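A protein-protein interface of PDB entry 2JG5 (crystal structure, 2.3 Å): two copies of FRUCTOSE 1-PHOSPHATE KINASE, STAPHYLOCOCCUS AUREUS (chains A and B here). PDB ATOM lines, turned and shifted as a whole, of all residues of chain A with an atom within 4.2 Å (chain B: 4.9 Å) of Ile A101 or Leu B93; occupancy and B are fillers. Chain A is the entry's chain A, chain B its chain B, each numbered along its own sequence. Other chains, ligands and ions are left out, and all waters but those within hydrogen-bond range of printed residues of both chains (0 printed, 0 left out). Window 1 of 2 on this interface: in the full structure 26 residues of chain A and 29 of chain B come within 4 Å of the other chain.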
ATOM      1  N   ASN A  90      23.192  -9.137  -7.019  1.00  0.00           N
ATOM      2  CA  ASN A  90      22.020  -8.558  -7.615  1.00  0.00           C
ATOM      3  C   ASN A  90      20.814  -9.392  -7.225  1.00  0.00           C
ATOM      4  O   ASN A  90      20.912 -10.613  -7.150  1.00  0.00           O
ATOM      5  CB  ASN A  90      22.179  -8.559  -9.128  1.00  0.00           C
ATOM      6  CG  ASN A  90      23.271  -7.630  -9.595  1.00  0.00           C
ATOM      7  OD1 ASN A  90      23.833  -6.868  -8.809  1.00  0.00           O
ATOM      8  ND2 ASN A  90      23.581  -7.685 -10.890  1.00  0.00           N
ATOM      9  N   VAL A  91      19.691  -8.737  -6.953  1.00  0.00           N
ATOM     10  CA  VAL A  91      18.485  -9.449  -6.519  1.00  0.00           C
ATOM     11  C   VAL A  91      17.406  -9.462  -7.606  1.00  0.00           C
ATOM     12  O   VAL A  91      17.103  -8.434  -8.189  1.00  0.00           O
ATOM     13  CB  VAL A  91      17.932  -8.897  -5.181  1.00  0.00           C
ATOM     14  CG1 VAL A  91      16.679  -9.652  -4.759  1.00  0.00           C
ATOM     15  CG2 VAL A  91      18.983  -9.001  -4.088  1.00  0.00           C
ATOM     16  N   THR A  99      11.099  -8.264 -10.718  1.00  0.00           N
ATOM     17  CA  THR A  99      11.664  -7.055 -10.148  1.00  0.00           C
ATOM     18  C   THR A  99      13.151  -7.255  -9.902  1.00  0.00           C
ATOM     19  O   THR A  99      13.526  -8.047  -9.056  1.00  0.00           O
ATOM     20  CB  THR A  99      10.940  -6.707  -8.820  1.00  0.00           C
ATOM     21  OG1 THR A  99       9.537  -6.543  -9.069  1.00  0.00           O
ATOM     22  CG2 THR A  99      11.489  -5.441  -8.209  1.00  0.00           C
ATOM     23  N   GLU A 100      13.990  -6.542 -10.651  1.00  0.00           N
ATOM     24  CA  GLU A 100      15.432  -6.611 -10.461  1.00  0.00           C
ATOM     25  C   GLU A 100      15.923  -5.507  -9.529  1.00  0.00           C
ATOM     26  O   GLU A 100      15.454  -4.373  -9.588  1.00  0.00           O
ATOM     27  CB  GLU A 100      16.163  -6.513 -11.801  1.00  0.00           C
ATOM     28  CG  GLU A 100      15.971  -7.697 -12.745  1.00  0.00           C
ATOM     29  CD  GLU A 100      16.933  -7.682 -13.941  1.00  0.00           C
ATOM     30  OE1 GLU A 100      17.926  -6.920 -13.922  1.00  0.00           O
ATOM     31  OE2 GLU A 100      16.697  -8.451 -14.906  1.00  0.00           O
ATOM     32  N   ILE A 101      16.860  -5.858  -8.658  1.00  0.00           N
ATOM     33  CA  ILE A 101      17.568  -4.892  -7.820  1.00  0.00           C
ATOM     34  C   ILE A 101      19.061  -5.094  -8.033  1.00  0.00           C
ATOM     35  O   ILE A 101      19.657  -6.039  -7.513  1.00  0.00           O
ATOM     36  CB  ILE A 101      17.224  -5.017  -6.306  1.00  0.00           C
ATOM     37  CG1 ILE A 101      15.707  -5.017  -6.094  1.00  0.00           C
ATOM     38  CG2 ILE A 101      17.885  -3.869  -5.510  1.00  0.00           C
ATOM     39  CD1 ILE A 101      15.273  -5.615  -4.778  1.00  0.00           C
ATOM     40  N   ASN A 102      19.648  -4.205  -8.827  1.00  0.00           N
ATOM     41  CA  ASN A 102      21.049  -4.273  -9.178  1.00  0.00           C
ATOM     42  C   ASN A 102      21.902  -3.415  -8.255  1.00  0.00           C
ATOM     43  O   ASN A 102      21.582  -2.250  -8.013  1.00  0.00           O
ATOM     44  CB  ASN A 102      21.234  -3.852 -10.633  1.00  0.00           C
ATOM     45  CG  ASN A 102      20.885  -4.962 -11.615  1.00  0.00           C
ATOM     46  OD1 ASN A 102      19.941  -5.735 -11.410  1.00  0.00           O
ATOM     47  ND2 ASN A 102      21.650  -5.039 -12.700  1.00  0.00           N
ATOM     48  N   ALA A 103      22.985  -4.016  -7.753  1.00  0.00           N
ATOM     49  CA  ALA A 103      23.882  -3.407  -6.764  1.00  0.00           C
ATOM     50  C   ALA A 103      25.076  -2.710  -7.425  1.00  0.00           C
ATOM     51  O   ALA A 103      25.382  -2.975  -8.593  1.00  0.00           O
ATOM     52  CB  ALA A 103      24.372  -4.466  -5.802  1.00  0.00           C
ATOM     53  N   ILE B  15      19.931  -3.085   1.734  1.00  0.00           N
ATOM     54  CA  ILE B  15      20.047  -2.490   0.419  1.00  0.00           C
ATOM     55  C   ILE B  15      19.311  -1.150   0.392  1.00  0.00           C
ATOM     56  O   ILE B  15      18.129  -1.074   0.701  1.00  0.00           O
ATOM     57  CB  ILE B  15      19.479  -3.454  -0.670  1.00  0.00           C
ATOM     58  CG1 ILE B  15      20.198  -4.810  -0.618  1.00  0.00           C
ATOM     59  CG2 ILE B  15      19.573  -2.844  -2.075  1.00  0.00           C
ATOM     60  CD1 ILE B  15      19.493  -5.923  -1.368  1.00  0.00           C
ATOM     61  N   THR B  17      18.214   1.813  -2.184  1.00  0.00           N
ATOM     62  CA  THR B  17      17.935   1.924  -3.612  1.00  0.00           C
ATOM     63  C   THR B  17      17.616   3.366  -4.001  1.00  0.00           C
ATOM     64  O   THR B  17      17.367   4.217  -3.147  1.00  0.00           O
ATOM     65  CB  THR B  17      16.750   1.016  -4.049  1.00  0.00           C
ATOM     66  OG1 THR B  17      15.560   1.397  -3.344  1.00  0.00           O
ATOM     67  CG2 THR B  17      17.042  -0.459  -3.796  1.00  0.00           C
ATOM     68  N   PHE B  20      12.003   2.891  -5.246  1.00  0.00           N
ATOM     69  CA  PHE B  20      11.648   1.511  -5.537  1.00  0.00           C
ATOM     70  C   PHE B  20      10.485   1.331  -6.492  1.00  0.00           C
ATOM     71  O   PHE B  20       9.469   2.040  -6.421  1.00  0.00           O
ATOM     72  CB  PHE B  20      11.442   0.688  -4.259  1.00  0.00           C
ATOM     73  CG  PHE B  20      11.641  -0.785  -4.468  1.00  0.00           C
ATOM     74  CD1 PHE B  20      12.866  -1.272  -4.901  1.00  0.00           C
ATOM     75  CD2 PHE B  20      10.597  -1.678  -4.276  1.00  0.00           C
ATOM     76  CE1 PHE B  20      13.054  -2.628  -5.122  1.00  0.00           C
ATOM     77  CE2 PHE B  20      10.776  -3.038  -4.488  1.00  0.00           C
ATOM     78  CZ  PHE B  20      12.003  -3.515  -4.912  1.00  0.00           C
ATOM     79  N   ASN B  26      15.621  -1.781 -10.771  1.00  0.00           N
ATOM     80  CA  ASN B  26      16.008  -0.908  -9.675  1.00  0.00           C
ATOM     81  C   ASN B  26      17.514  -0.967  -9.502  1.00  0.00           C
ATOM     82  O   ASN B  26      18.114  -2.047  -9.579  1.00  0.00           O
ATOM     83  CB  ASN B  26      15.326  -1.349  -8.372  1.00  0.00           C
ATOM     84  CG  ASN B  26      13.822  -1.100  -8.381  1.00  0.00           C
ATOM     85  OD1 ASN B  26      13.357  -0.058  -7.913  1.00  0.00           O
ATOM     86  ND2 ASN B  26      13.056  -2.045  -8.927  1.00  0.00           N
ATOM     87  N   ALA B  28      20.487  -0.361  -6.772  1.00  0.00           N
ATOM     88  CA  ALA B  28      20.875  -0.133  -5.395  1.00  0.00           C
ATOM     89  C   ALA B  28      22.016   0.851  -5.428  1.00  0.00           C
ATOM     90  O   ALA B  28      22.901   0.747  -6.276  1.00  0.00           O
ATOM     91  CB  ALA B  28      21.319  -1.431  -4.740  1.00  0.00           C
ATOM     92  N   VAL B  91      17.150 -10.380   2.811  1.00  0.00           N
ATOM     93  CA  VAL B  91      17.226  -9.060   2.192  1.00  0.00           C
ATOM     94  C   VAL B  91      16.348  -8.071   2.947  1.00  0.00           C
ATOM     95  O   VAL B  91      15.170  -8.336   3.227  1.00  0.00           O
ATOM     96  CB  VAL B  91      16.820  -9.119   0.686  1.00  0.00           C
ATOM     97  CG1 VAL B  91      16.730  -7.720   0.073  1.00  0.00           C
ATOM     98  CG2 VAL B  91      17.792 -10.004  -0.098  1.00  0.00           C
ATOM     99  N   LYS B  92      16.939  -6.931   3.288  1.00  0.00           N
ATOM    100  CA  LYS B  92      16.197  -5.847   3.920  1.00  0.00           C
ATOM    101  C   LYS B  92      16.303  -4.619   3.040  1.00  0.00           C
ATOM    102  O   LYS B  92      17.403  -4.116   2.799  1.00  0.00           O
ATOM    103  CB  LYS B  92      16.740  -5.562   5.324  1.00  0.00           C
ATOM    104  CG  LYS B  92      16.277  -6.550   6.397  1.00  0.00           C
ATOM    105  CD  LYS B  92      17.146  -7.821   6.454  1.00  0.00           C
ATOM    106  CE  LYS B  92      16.659  -8.802   7.529  1.00  0.00           C
ATOM    107  NZ  LYS B  92      16.506  -8.153   8.879  1.00  0.00           N
ATOM    108  N   LEU B  93      15.164  -4.155   2.536  1.00  0.00           N
ATOM    109  CA  LEU B  93      15.130  -2.996   1.658  1.00  0.00           C
ATOM    110  C   LEU B  93      14.737  -1.772   2.465  1.00  0.00           C
ATOM    111  O   LEU B  93      13.667  -1.736   3.077  1.00  0.00           O
ATOM    112  CB  LEU B  93      14.148  -3.215   0.512  1.00  0.00           C
ATOM    113  CG  LEU B  93      14.381  -4.370  -0.464  1.00  0.00           C
ATOM    114  CD1 LEU B  93      13.252  -4.413  -1.502  1.00  0.00           C
ATOM    115  CD2 LEU B  93      15.737  -4.262  -1.140  1.00  0.00           C
ATOM    116  N   LYS B  94      15.605  -0.767   2.451  1.00  0.00           N
ATOM    117  CA  LYS B  94      15.484   0.373   3.365  1.00  0.00           C
ATOM    118  C   LYS B  94      15.103   1.713   2.719  1.00  0.00           C
ATOM    119  O   LYS B  94      14.909   2.698   3.432  1.00  0.00           O
ATOM    120  CB  LYS B  94      16.771   0.532   4.189  1.00  0.00           C
ATOM    121  CG  LYS B  94      17.096  -0.629   5.152  1.00  0.00           C
ATOM    122  CD  LYS B  94      16.157  -0.681   6.368  1.00  0.00           C
ATOM    123  CE  LYS B  94      16.153   0.640   7.164  1.00  0.00           C
ATOM    124  NZ  LYS B  94      14.874   0.857   7.900  1.00  0.00           N
ATOM    125  N   THR B  95      14.990   1.764   1.392  1.00  0.00           N
ATOM    126  CA  THR B  95      14.679   3.033   0.717  1.00  0.00           C
ATOM    127  C   THR B  95      13.177   3.283   0.590  1.00  0.00           C
ATOM    128  O   THR B  95      12.458   2.552  -0.106  1.00  0.00           O
ATOM    129  CB  THR B  95      15.386   3.185  -0.643  1.00  0.00           C
ATOM    130  OG1 THR B  95      16.799   3.237  -0.428  1.00  0.00           O
ATOM    131  CG2 THR B  95      14.941   4.477  -1.353  1.00  0.00           C
ATOM    132  N   GLN B  97       9.965   2.643   1.791  1.00  0.00           N
ATOM    133  CA  GLN B  97       9.301   1.629   2.586  1.00  0.00           C
ATOM    134  C   GLN B  97      10.276   0.504   2.956  1.00  0.00           C
ATOM    135  O   GLN B  97      11.021   0.007   2.101  1.00  0.00           O
ATOM    136  CB  GLN B  97       8.058   1.112   1.854  1.00  0.00           C
ATOM    137  CG  GLN B  97       6.871   2.111   1.809  1.00  0.00           C
ATOM    138  CD  GLN B  97       6.912   3.071   0.611  1.00  0.00           C
ATOM    139  OE1 GLN B  97       7.919   3.743   0.361  1.00  0.00           O
ATOM    140  NE2 GLN B  97       5.802   3.144  -0.125  1.00  0.00           N
ATOM    141  N   GLU B  98      10.284   0.136   4.237  1.00  0.00           N
ATOM    142  CA  GLU B  98      11.253  -0.827   4.765  1.00  0.00           C
ATOM    143  C   GLU B  98      10.732  -2.271   4.825  1.00  0.00           C
ATOM    144  O   GLU B  98       9.895  -2.634   5.659  1.00  0.00           O
ATOM    145  CB  GLU B  98      11.883  -0.330   6.077  1.00  0.00           C
ATOM    146  CG  GLU B  98      11.000  -0.325   7.301  1.00  0.00           C
ATOM    147  CD  GLU B  98      11.324  -1.473   8.235  1.00  0.00           C
ATOM    148  OE1 GLU B  98      12.415  -2.075   8.095  1.00  0.00           O
ATOM    149  OE2 GLU B  98      10.492  -1.772   9.116  1.00  0.00           O
ATOM    150  N   THR B  99      11.255  -3.074   3.900  1.00  0.00           N
ATOM    151  CA  THR B  99      10.686  -4.357   3.530  1.00  0.00           C
ATOM    152  C   THR B  99      11.681  -5.478   3.772  1.00  0.00           C
ATOM    153  O   THR B  99      12.867  -5.331   3.517  1.00  0.00           O
ATOM    154  CB  THR B  99      10.295  -4.358   2.039  1.00  0.00           C
ATOM    155  OG1 THR B  99       9.496  -3.207   1.744  1.00  0.00           O
ATOM    156  CG2 THR B  99       9.523  -5.629   1.667  1.00  0.00           C
ATOM    157  N   ILE B 101      12.776  -9.619   3.266  1.00  0.00           N
ATOM    158  CA  ILE B 101      12.612 -10.773   2.391  1.00  0.00           C
ATOM    159  C   ILE B 101      13.463 -11.929   2.888  1.00  0.00           C
ATOM    160  O   ILE B 101      14.649 -12.018   2.579  1.00  0.00           O
ATOM    161  CB  ILE B 101      12.949 -10.448   0.917  1.00  0.00           C
ATOM    162  CG1 ILE B 101      12.267  -9.141   0.471  1.00  0.00           C
ATOM    163  CG2 ILE B 101      12.504 -11.601   0.011  1.00  0.00           C
ATOM    164  CD1 ILE B 101      13.092  -8.290  -0.487  1.00  0.00           C
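The side-chain amide oxygen (OD1) of Asn A90 is in hydrogen-bond range of the backbone NH (N) of Ala A103, at 3.2 Å.
O of Ile B15 lies within hydrogen-bond range of N of Lys B94 (3.1 Å).
OE1 of Glu A100 sits close to OD1 of Asn A102 (3.4 Å).
O of Lys B92 lies within hydrogen-bond range of N of Ile B15.
The backbone carbonyl oxygen (O) of Thr B99 sits at hydrogen-bond distance from the backbone NH (N) of Leu B93, at 2.8 Å.
N of Ile A101 lies within hydrogen-bond range of O of Val A91.
Printed residues of chain A that touch a printed residue of chain B: Thr A99, Glu A100, Ile A101, Asn A102 and Ala A103.
Printed residues of chain B that touch a printed residue of chain A: Ile B15, Thr B17, Phe B20, Asn B26, Ala B28 and Leu B93.
Among the printed residues, 11 pairs touch across the chains.
Among the printed residues, no Asp or Glu carboxylate lies within 4 Å of a Lys or Arg side-chain nitrogen of the other chain.
Of the printed residues of chain B, Ile A101 touches Ile B15 (3.96 Å), Thr B17 (3.9 Å), Phe B20 (3.7 Å), Asn B26 (3.4 Å) and Leu B93 (3.9 Å).
Of the printed residues of chain A, Ile B15 touches Ile A101 (3.96 Å).
Of the printed residues of chain A, Phe B20 touches Thr A99 and Ile A101.
Leu B93 touches one residue of chain A.
Lys B94 touches none of the printed residues of chain A.
Glu B98 touches none of the printed residues of chain A.
The nearest residue of chain B that does not touch Ile A101 is Ala B28 (4.3 Å).
The nearest printed residue of chain A that does not touch Thr B17 is Asn A102 (6.4 Å).
3 positions are printed for both chains.
Of the 11 pairs that touch across the chains among the printed residues, none has its exchanged pair printed and touching as well.
O of Asn A102 sits at hydrogen-bond distance from N of Ala B28, 2.5 Å away.
The backbone NH (N) of Asn A102 lies within hydrogen-bond range of the backbone carbonyl oxygen (O) of Asn B26 (2.8 Å).
The backbone carbonyl oxygen (O) of Glu A100 lies within hydrogen-bond range of the backbone NH (N) of Asn B26 (2.9 Å).
Among the printed residues, pairs that only touch across the chains: Thr A99 with Phe B20 (3.9 Å), Thr A99 with Asn B26 (3.8 Å), Ile A101 with Ile B15 (3.96 Å), Ile A101 with Thr B17 (3.9 Å), Ile A101 with Phe B20 (3.7 Å), Ile A101 with Asn B26 (3.4 Å), Ile A101 with Leu B93 (3.9 Å) and Ala A103 with Ala B28 (3.8 Å).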
